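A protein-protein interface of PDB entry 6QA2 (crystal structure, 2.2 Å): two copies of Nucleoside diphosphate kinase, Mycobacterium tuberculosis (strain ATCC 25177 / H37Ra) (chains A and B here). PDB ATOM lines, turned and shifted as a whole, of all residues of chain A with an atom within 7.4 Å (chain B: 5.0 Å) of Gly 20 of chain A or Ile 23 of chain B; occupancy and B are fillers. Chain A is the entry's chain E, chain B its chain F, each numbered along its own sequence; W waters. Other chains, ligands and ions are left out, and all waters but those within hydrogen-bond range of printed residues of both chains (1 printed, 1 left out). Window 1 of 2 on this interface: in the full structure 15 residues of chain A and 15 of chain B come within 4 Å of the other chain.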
ATOM      1  N   ILE A   9      -2.714  17.313 -25.381  1.00  0.00           N
ATOM      2  CA  ILE A   9      -1.593  17.943 -26.066  1.00  0.00           C
ATOM      3  C   ILE A   9      -0.343  17.179 -25.645  1.00  0.00           C
ATOM      4  O   ILE A   9       0.088  17.262 -24.492  1.00  0.00           O
ATOM      5  CB  ILE A   9      -1.486  19.435 -25.738  1.00  0.00           C
ATOM      6  CG1 ILE A   9      -2.805  20.142 -26.069  1.00  0.00           C
ATOM      7  CG2 ILE A   9      -0.345  20.070 -26.524  1.00  0.00           C
ATOM      8  CD1 ILE A   9      -2.803  21.633 -25.780  1.00  0.00           C
ATOM      9  N   GLY A  13       3.942  18.722 -28.172  1.00  0.00           N
ATOM     10  CA  GLY A  13       3.148  19.928 -28.330  1.00  0.00           C
ATOM     11  C   GLY A  13       3.501  20.997 -27.314  1.00  0.00           C
ATOM     12  O   GLY A  13       3.473  22.192 -27.622  1.00  0.00           O
ATOM     13  N   GLN A  17       5.786  24.800 -27.728  1.00  0.00           N
ATOM     14  CA  GLN A  17       5.019  25.963 -27.286  1.00  0.00           C
ATOM     15  C   GLN A  17       3.817  26.208 -28.193  1.00  0.00           C
ATOM     16  O   GLN A  17       3.607  27.305 -28.714  1.00  0.00           O
ATOM     17  CB  GLN A  17       5.914  27.201 -27.213  1.00  0.00           C
ATOM     18  CG  GLN A  17       6.967  27.133 -26.117  1.00  0.00           C
ATOM     19  CD  GLN A  17       7.817  28.386 -26.050  1.00  0.00           C
ATOM     20  OE1 GLN A  17       7.793  29.112 -25.055  1.00  0.00           O
ATOM     21  NE2 GLN A  17       8.574  28.647 -27.111  1.00  0.00           N
ATOM     22  N   LEU A  18       3.015  25.159 -28.377  1.00  0.00           N
ATOM     23  CA  LEU A  18       1.819  25.220 -29.207  1.00  0.00           C
ATOM     24  C   LEU A  18       0.540  25.032 -28.394  1.00  0.00           C
ATOM     25  O   LEU A  18      -0.510  24.718 -28.965  1.00  0.00           O
ATOM     26  CB  LEU A  18       1.898  24.173 -30.318  1.00  0.00           C
ATOM     27  CG  LEU A  18       2.917  24.451 -31.426  1.00  0.00           C
ATOM     28  CD1 LEU A  18       3.140  23.212 -32.279  1.00  0.00           C
ATOM     29  CD2 LEU A  18       2.462  25.618 -32.290  1.00  0.00           C
ATOM     30  N   ILE A  19       0.605  25.220 -27.073  1.00  0.00           N
ATOM     31  CA  ILE A  19      -0.586  25.069 -26.240  1.00  0.00           C
ATOM     32  C   ILE A  19      -1.660  26.062 -26.667  1.00  0.00           C
ATOM     33  O   ILE A  19      -2.803  25.687 -26.951  1.00  0.00           O
ATOM     34  CB  ILE A  19      -0.235  25.241 -24.751  1.00  0.00           C
ATOM     35  CG1 ILE A  19       0.726  24.143 -24.288  1.00  0.00           C
ATOM     36  CG2 ILE A  19      -1.508  25.237 -23.909  1.00  0.00           C
ATOM     37  CD1 ILE A  19       1.305  24.387 -22.906  1.00  0.00           C
ATOM     38  N   GLY A  20      -1.309  27.350 -26.706  1.00  0.00           N
ATOM     39  CA  GLY A  20      -2.296  28.365 -27.034  1.00  0.00           C
ATOM     40  C   GLY A  20      -2.849  28.208 -28.435  1.00  0.00           C
ATOM     41  O   GLY A  20      -4.049  28.383 -28.665  1.00  0.00           O
ATOM     42  N   GLU A  21      -1.982  27.875 -29.393  1.00  0.00           N
ATOM     43  CA  GLU A  21      -2.431  27.679 -30.766  1.00  0.00           C
ATOM     44  C   GLU A  21      -3.459  26.557 -30.853  1.00  0.00           C
ATOM     45  O   GLU A  21      -4.492  26.701 -31.518  1.00  0.00           O
ATOM     46  CB  GLU A  21      -1.230  27.381 -31.663  1.00  0.00           C
ATOM     47  CG  GLU A  21      -1.555  27.267 -33.142  1.00  0.00           C
ATOM     48  CD  GLU A  21      -2.102  28.555 -33.726  1.00  0.00           C
ATOM     49  OE1 GLU A  21      -3.305  28.596 -34.062  1.00  0.00           O
ATOM     50  OE2 GLU A  21      -1.327  29.529 -33.843  1.00  0.00           O
ATOM     51  N   ILE A  22      -3.200  25.434 -30.181  1.00  0.00           N
ATOM     52  CA  ILE A  22      -4.131  24.312 -30.228  1.00  0.00           C
ATOM     53  C   ILE A  22      -5.448  24.681 -29.560  1.00  0.00           C
ATOM     54  O   ILE A  22      -6.529  24.365 -30.072  1.00  0.00           O
ATOM     55  CB  ILE A  22      -3.493  23.066 -29.587  1.00  0.00           C
ATOM     56  CG1 ILE A  22      -2.409  22.499 -30.510  1.00  0.00           C
ATOM     57  CG2 ILE A  22      -4.557  22.017 -29.281  1.00  0.00           C
ATOM     58  CD1 ILE A  22      -1.585  21.391 -29.892  1.00  0.00           C
ATOM     59  N   ILE A  23      -5.387  25.356 -28.410  1.00  0.00           N
ATOM     60  CA  ILE A  23      -6.610  25.731 -27.707  1.00  0.00           C
ATOM     61  C   ILE A  23      -7.375  26.792 -28.490  1.00  0.00           C
ATOM     62  O   ILE A  23      -8.612  26.801 -28.501  1.00  0.00           O
ATOM     63  CB  ILE A  23      -6.280  26.206 -26.281  1.00  0.00           C
ATOM     64  CG1 ILE A  23      -5.697  25.048 -25.465  1.00  0.00           C
ATOM     65  CG2 ILE A  23      -7.530  26.778 -25.616  1.00  0.00           C
ATOM     66  CD1 ILE A  23      -5.177  25.446 -24.097  1.00  0.00           C
ATOM     67  N   SER A  24      -6.659  27.706 -29.151  1.00  0.00           N
ATOM     68  CA  SER A  24      -7.325  28.709 -29.977  1.00  0.00           C
ATOM     69  C   SER A  24      -8.186  28.051 -31.046  1.00  0.00           C
ATOM     70  O   SER A  24      -9.338  28.442 -31.262  1.00  0.00           O
ATOM     71  CB  SER A  24      -6.291  29.634 -30.624  1.00  0.00           C
ATOM     72  OG  SER A  24      -5.659  30.455 -29.659  1.00  0.00           O
ATOM     73  N   ARG A  25      -7.639  27.042 -31.728  1.00  0.00           N
ATOM     74  CA  ARG A  25      -8.390  26.372 -32.784  1.00  0.00           C
ATOM     75  C   ARG A  25      -9.613  25.655 -32.235  1.00  0.00           C
ATOM     76  O   ARG A  25     -10.647  25.587 -32.910  1.00  0.00           O
ATOM     77  CB  ARG A  25      -7.487  25.390 -33.521  1.00  0.00           C
ATOM     78  CG  ARG A  25      -6.347  26.061 -34.252  1.00  0.00           C
ATOM     79  CD  ARG A  25      -5.873  25.205 -35.395  1.00  0.00           C
ATOM     80  NE  ARG A  25      -4.861  25.879 -36.197  1.00  0.00           N
ATOM     81  CZ  ARG A  25      -4.440  25.445 -37.379  1.00  0.00           C
ATOM     82  NH1 ARG A  25      -4.949  24.336 -37.899  1.00  0.00           N
ATOM     83  NH2 ARG A  25      -3.513  26.123 -38.041  1.00  0.00           N
ATOM     84  N   ILE A  26      -9.514  25.107 -31.024  1.00  0.00           N
ATOM     85  CA  ILE A  26     -10.670  24.478 -30.400  1.00  0.00           C
ATOM     86  C   ILE A  26     -11.744  25.517 -30.106  1.00  0.00           C
ATOM     87  O   ILE A  26     -12.932  25.293 -30.368  1.00  0.00           O
ATOM     88  CB  ILE A  26     -10.237  23.731 -29.125  1.00  0.00           C
ATOM     89  CG1 ILE A  26      -9.356  22.533 -29.493  1.00  0.00           C
ATOM     90  CG2 ILE A  26     -11.455  23.289 -28.327  1.00  0.00           C
ATOM     91  CD1 ILE A  26      -8.615  21.925 -28.317  1.00  0.00           C
ATOM     92  N   GLU A  27     -11.344  26.676 -29.578  1.00  0.00           N
ATOM     93  CA  GLU A  27     -12.313  27.690 -29.180  1.00  0.00           C
ATOM     94  C   GLU A  27     -12.997  28.325 -30.386  1.00  0.00           C
ATOM     95  O   GLU A  27     -14.221  28.496 -30.392  1.00  0.00           O
ATOM     96  CB  GLU A  27     -11.628  28.755 -28.327  1.00  0.00           C
ATOM     97  CG  GLU A  27     -11.298  28.294 -26.915  1.00  0.00           C
ATOM     98  CD  GLU A  27     -10.542  29.339 -26.121  1.00  0.00           C
ATOM     99  OE1 GLU A  27      -9.554  29.892 -26.647  1.00  0.00           O
ATOM    100  OE2 GLU A  27     -10.942  29.611 -24.970  1.00  0.00           O
ATOM    101  N   LEU A  36      -9.076  21.566 -17.931  1.00  0.00           N
ATOM    102  CA  LEU A  36      -7.755  21.857 -18.474  1.00  0.00           C
ATOM    103  C   LEU A  36      -6.732  21.679 -17.367  1.00  0.00           C
ATOM    104  O   LEU A  36      -6.939  22.169 -16.253  1.00  0.00           O
ATOM    105  CB  LEU A  36      -7.697  23.285 -19.033  1.00  0.00           C
ATOM    106  CG  LEU A  36      -6.386  23.714 -19.693  1.00  0.00           C
ATOM    107  CD1 LEU A  36      -6.178  22.970 -21.002  1.00  0.00           C
ATOM    108  CD2 LEU A  36      -6.369  25.220 -19.918  1.00  0.00           C
ATOM    109  N   ILE B   9      -6.348  34.060 -16.064  1.00  0.00           N
ATOM    110  CA  ILE B   9      -7.312  34.447 -17.087  1.00  0.00           C
ATOM    111  C   ILE B   9      -8.655  34.592 -16.379  1.00  0.00           C
ATOM    112  O   ILE B   9      -9.232  33.606 -15.913  1.00  0.00           O
ATOM    113  CB  ILE B   9      -7.378  33.427 -18.228  1.00  0.00           C
ATOM    114  CG1 ILE B   9      -5.971  33.172 -18.781  1.00  0.00           C
ATOM    115  CG2 ILE B   9      -8.306  33.928 -19.330  1.00  0.00           C
ATOM    116  CD1 ILE B   9      -5.931  32.274 -20.004  1.00  0.00           C
ATOM    117  N   ILE B  19      -8.866  31.923 -24.205  1.00  0.00           N
ATOM    118  CA  ILE B  19      -7.845  31.213 -23.440  1.00  0.00           C
ATOM    119  C   ILE B  19      -6.607  30.979 -24.298  1.00  0.00           C
ATOM    120  O   ILE B  19      -5.485  31.326 -23.910  1.00  0.00           O
ATOM    121  CB  ILE B  19      -8.406  29.890 -22.889  1.00  0.00           C
ATOM    122  CG1 ILE B  19      -9.562  30.165 -21.924  1.00  0.00           C
ATOM    123  CG2 ILE B  19      -7.301  29.095 -22.193  1.00  0.00           C
ATOM    124  CD1 ILE B  19     -10.324  28.925 -21.499  1.00  0.00           C
ATOM    125  N   GLY B  20      -6.791  30.381 -25.477  1.00  0.00           N
ATOM    126  CA  GLY B  20      -5.652  30.070 -26.323  1.00  0.00           C
ATOM    127  C   GLY B  20      -4.932  31.310 -26.816  1.00  0.00           C
ATOM    128  O   GLY B  20      -3.701  31.345 -26.872  1.00  0.00           O
ATOM    129  N   GLU B  21      -5.690  32.345 -27.182  1.00  0.00           N
ATOM    130  CA  GLU B  21      -5.077  33.579 -27.663  1.00  0.00           C
ATOM    131  C   GLU B  21      -4.165  34.190 -26.606  1.00  0.00           C
ATOM    132  O   GLU B  21      -3.089  34.708 -26.927  1.00  0.00           O
ATOM    133  CB  GLU B  21      -6.166  34.570 -28.073  1.00  0.00           C
ATOM    134  CG  GLU B  21      -5.636  35.869 -28.652  1.00  0.00           C
ATOM    135  CD  GLU B  21      -4.872  35.663 -29.942  1.00  0.00           C
ATOM    136  OE1 GLU B  21      -5.443  35.067 -30.880  1.00  0.00           O
ATOM    137  OE2 GLU B  21      -3.699  36.090 -30.015  1.00  0.00           O
ATOM    138  N   ILE B  22      -4.578  34.141 -25.340  1.00  0.00           N
ATOM    139  CA  ILE B  22      -3.764  34.706 -24.269  1.00  0.00           C
ATOM    140  C   ILE B  22      -2.528  33.845 -24.026  1.00  0.00           C
ATOM    141  O   ILE B  22      -1.420  34.364 -23.841  1.00  0.00           O
ATOM    142  CB  ILE B  22      -4.613  34.870 -22.995  1.00  0.00           C
ATOM    143  CG1 ILE B  22      -5.590  36.038 -23.167  1.00  0.00           C
ATOM    144  CG2 ILE B  22      -3.722  35.085 -21.776  1.00  0.00           C
ATOM    145  CD1 ILE B  22      -6.665  36.115 -22.106  1.00  0.00           C
ATOM    146  N   ILE B  23      -2.691  32.521 -24.026  1.00  0.00           N
ATOM    147  CA  ILE B  23      -1.545  31.634 -23.846  1.00  0.00           C
ATOM    148  C   ILE B  23      -0.574  31.773 -25.012  1.00  0.00           C
ATOM    149  O   ILE B  23       0.648  31.745 -24.827  1.00  0.00           O
ATOM    150  CB  ILE B  23      -2.017  30.179 -23.671  1.00  0.00           C
ATOM    151  CG1 ILE B  23      -2.782  30.031 -22.353  1.00  0.00           C
ATOM    152  CG2 ILE B  23      -0.827  29.222 -23.720  1.00  0.00           C
ATOM    153  CD1 ILE B  23      -3.462  28.687 -22.176  1.00  0.00           C
ATOM    154  N   SER B  24      -1.098  31.925 -26.230  1.00  0.00           N
ATOM    155  CA  SER B  24      -0.228  32.049 -27.396  1.00  0.00           C
ATOM    156  C   SER B  24       0.696  33.253 -27.272  1.00  0.00           C
ATOM    157  O   SER B  24       1.888  33.165 -27.588  1.00  0.00           O
ATOM    158  CB  SER B  24      -1.066  32.152 -28.670  1.00  0.00           C
ATOM    159  OG  SER B  24      -1.841  30.984 -28.859  1.00  0.00           O
ATOM    160  N   ARG B  25       0.166  34.391 -26.817  1.00  0.00           N
ATOM    161  CA  ARG B  25       0.996  35.582 -26.673  1.00  0.00           C
ATOM    162  C   ARG B  25       2.051  35.400 -25.590  1.00  0.00           C
ATOM    163  O   ARG B  25       3.153  35.948 -25.703  1.00  0.00           O
ATOM    164  CB  ARG B  25       0.119  36.796 -26.375  1.00  0.00           C
ATOM    165  CG  ARG B  25      -0.499  37.426 -27.617  1.00  0.00           C
ATOM    166  CD  ARG B  25      -1.687  38.290 -27.249  1.00  0.00           C
ATOM    167  NE  ARG B  25      -2.318  38.911 -28.413  1.00  0.00           N
ATOM    168  CZ  ARG B  25      -2.251  40.206 -28.719  1.00  0.00           C
ATOM    169  NH1 ARG B  25      -1.578  41.060 -27.955  1.00  0.00           N
ATOM    170  NH2 ARG B  25      -2.873  40.656 -29.800  1.00  0.00           N
ATOM    171  N   ILE B  26       1.736  34.642 -24.538  1.00  0.00           N
ATOM    172  CA  ILE B  26       2.744  34.306 -23.540  1.00  0.00           C
ATOM    173  C   ILE B  26       3.801  33.393 -24.146  1.00  0.00           C
ATOM    174  O   ILE B  26       5.002  33.567 -23.912  1.00  0.00           O
ATOM    175  CB  ILE B  26       2.085  33.658 -22.309  1.00  0.00           C
ATOM    176  CG1 ILE B  26       1.084  34.618 -21.662  1.00  0.00           C
ATOM    177  CG2 ILE B  26       3.145  33.233 -21.300  1.00  0.00           C
ATOM    178  CD1 ILE B  26       0.222  33.969 -20.593  1.00  0.00           C
ATOM    179  N   GLU B  27       3.371  32.410 -24.941  1.00  0.00           N
ATOM    180  CA  GLU B  27       4.299  31.422 -25.483  1.00  0.00           C
ATOM    181  C   GLU B  27       5.217  32.029 -26.535  1.00  0.00           C
ATOM    182  O   GLU B  27       6.423  31.752 -26.546  1.00  0.00           O
ATOM    183  CB  GLU B  27       3.519  30.245 -26.068  1.00  0.00           C
ATOM    184  CG  GLU B  27       2.978  29.282 -25.023  1.00  0.00           C
ATOM    185  CD  GLU B  27       2.144  28.171 -25.630  1.00  0.00           C
ATOM    186  OE1 GLU B  27       1.291  28.472 -26.493  1.00  0.00           O
ATOM    187  OE2 GLU B  27       2.347  26.996 -25.253  1.00  0.00           O
ATOM    188  N   ARG B  28       4.674  32.851 -27.435  1.00  0.00           N
ATOM    189  CA  ARG B  28       5.504  33.438 -28.480  1.00  0.00           C
ATOM    190  C   ARG B  28       6.457  34.490 -27.930  1.00  0.00           C
ATOM    191  O   ARG B  28       7.462  34.798 -28.577  1.00  0.00           O
ATOM    192  CB  ARG B  28       4.630  34.051 -29.573  1.00  0.00           C
ATOM    193  CG  ARG B  28       3.988  35.359 -29.179  1.00  0.00           C
ATOM    194  CD  ARG B  28       3.075  35.863 -30.273  1.00  0.00           C
ATOM    195  NE  ARG B  28       2.537  37.178 -29.952  1.00  0.00           N
ATOM    196  CZ  ARG B  28       1.843  37.922 -30.803  1.00  0.00           C
ATOM    197  NH1 ARG B  28       1.608  37.476 -32.029  1.00  0.00           N
ATOM    198  NH2 ARG B  28       1.388  39.111 -30.430  1.00  0.00           N
ATOM    199  N   ILE B  33       5.028  27.650 -20.131  1.00  0.00           N
ATOM    200  CA  ILE B  33       3.906  27.340 -19.253  1.00  0.00           C
ATOM    201  C   ILE B  33       4.352  26.196 -18.347  1.00  0.00           C
ATOM    202  O   ILE B  33       4.403  25.039 -18.766  1.00  0.00           O
ATOM    203  CB  ILE B  33       2.650  26.977 -20.046  1.00  0.00           C
ATOM    204  CG1 ILE B  33       2.318  28.072 -21.067  1.00  0.00           C
ATOM    205  CG2 ILE B  33       1.474  26.750 -19.106  1.00  0.00           C
ATOM    206  CD1 ILE B  33       2.081  29.443 -20.462  1.00  0.00           C
ATOM    207  N   LEU B  36      -0.676  24.896 -15.308  1.00  0.00           N
ATOM    208  CA  LEU B  36      -1.873  25.335 -16.013  1.00  0.00           C
ATOM    209  C   LEU B  36      -3.058  24.540 -15.491  1.00  0.00           C
ATOM    210  O   LEU B  36      -2.977  23.313 -15.383  1.00  0.00           O
ATOM    211  CB  LEU B  36      -1.711  25.134 -17.524  1.00  0.00           C
ATOM    212  CG  LEU B  36      -2.836  25.644 -18.423  1.00  0.00           C
ATOM    213  CD1 LEU B  36      -2.911  27.160 -18.382  1.00  0.00           C
ATOM    214  CD2 LEU B  36      -2.633  25.148 -19.848  1.00  0.00           C
HETATM  215  O   HOH W   1       0.821  28.495 -28.897  1.00  0.00           O
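OE1 of Gln 17 of chain A sits close to O of Glu 27 of chain B (3.3 Å).
The backbone NH of Ile 19 of chain A sits at hydrogen-bond distance from the side-chain carboxylate of Glu 27 of chain B, at 3.1 Å.
The backbone carbonyl oxygen (O) of Gly 20 of chain A lies close to the side-chain hydroxyl (OG) of Ser 24 of chain B (3.4 Å).
The backbone NH (N) of Gly 20 of chain A lies within hydrogen-bond range of the side-chain carboxylate (OE1) of Glu 27 of chain B (2.8 Å).
N of Glu 21 of chain A is in hydrogen-bond range of OG of Ser 24 of chain B, 3.2 Å away.
OG of Ser 24 of chain A is in hydrogen-bond range of N of Glu 21 of chain B (3.1 Å).
The backbone NH (N) of Ile 19 of chain B lies within hydrogen-bond range of the side-chain carboxylate (OE2) of Glu 27 of chain A (3.2 Å).
The backbone NH of Gly 20 of chain B sits at hydrogen-bond distance from the side-chain carboxylate of Glu 27 of chain A (3.0 Å).
The backbone carbonyl oxygen (O) of Gly 20 of chain A sits close to the backbone carbonyl oxygen (O) of Gly 20 of chain B.
The backbone NH of Leu 18 of chain A is in hydrogen-bond range of the backbone carbonyl oxygen of Gly 13 of chain A (3.1 Å).
The side-chain hydroxyl (OG) of Ser 24 of chain A is in hydrogen-bond range of the backbone carbonyl oxygen (O) of Gly 20 of chain A (2.8 Å).
The guanidinium group of Arg 25 of chain A lies within salt-bridge range of the side-chain carboxylate of Glu 21 of chain A (3.8 Å).
The backbone carbonyl oxygen of Gly 20 of chain B sits at hydrogen-bond distance from the side-chain hydroxyl of Ser 24 of chain B, 2.7 Å away.
The side-chain carboxylate (OE2) of Glu 21 of chain B lies within salt-bridge range of the guanidinium group (NE) of Arg 25 of chain B (3.5 Å).
Among the printed residues, pairs that only touch across the chains: Ser 24 of chain A with Gly 20 of chain B (3.1 Å), Gly 20 of chain A with Ile 23 of chain B (3.6 Å), Ile 23 of chain A with Gly 20 of chain B (3.7 Å), Leu 18 of chain A with Glu 27 of chain B (3.7 Å), Leu 36 of chain A with Leu 36 of chain B (3.7 Å) and Ser 24 of chain A with Ser 24 of chain B (3.9 Å).
Ile 23 of chain B touches one residue of chain A.
Printed residues of chain A within 4 Å of Leu 36 of chain B: Leu 36.
Of the printed residues of chain B, Ile 19 of chain A touches Glu 27 (3.1 Å).
Of the printed residues of chain A, Gly 20 of chain B touches Gly 20, Ile 23, Ser 24 and Glu 27.
Arg 28 of chain B touches none of the printed residues of chain A.
Ile 9 of chain B touches none of the printed residues of chain A.
The nearest residue of chain B that does not touch Gly 20 of chain A is Glu 21 of chain B (4.5 Å).
The nearest printed residue of chain B that does not touch Glu 27 of chain A is Glu 21 of chain B (4.6 Å).
Of the 13 printed residues of chain B, 7 touch a printed residue of chain A.
Hydrophobic or aromatic side chains of chain B that line the printed part of chain A: Ile 19, Ile 23 and Leu 36.
Hydrophobic or aromatic side chains of chain A that line the printed part of chain B: Ile 19, Ile 23 and Leu 36.
Among the printed residues, 15 pairs touch across the chains.
Among the printed residues, no Asp or Glu carboxylate lies within 4 Å of a Lys or Arg side-chain nitrogen of the other chain.
Ile 19 of chain A touches Glu 27 of chain B, and with the chains exchanged Glu 27 of chain A touches Ile 19 of chain B.
Gly 20 of chain A touches Ser 24 of chain B, and with the chains exchanged Ser 24 of chain A touches Gly 20 of chain B.
Gly 20 of chain A touches Glu 27 of chain B, and with the chains exchanged Glu 27 of chain A touches Gly 20 of chain B.
Leu 36 of chain A touches its own counterpart, Leu 36 of chain B.
Positions printed for both chains: 9, 19, 20, 21, 22, 23, 24, 25, 26, 27 and 36.
Water W1 lies within hydrogen-bond range of OE1 of Glu 27 of chain B (2.4 Å), N of Glu 21 of chain A (2.9 Å), O of Gln 17 of chain A (3.0 Å) and N of Gly 20 of chain A (3.3 Å).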
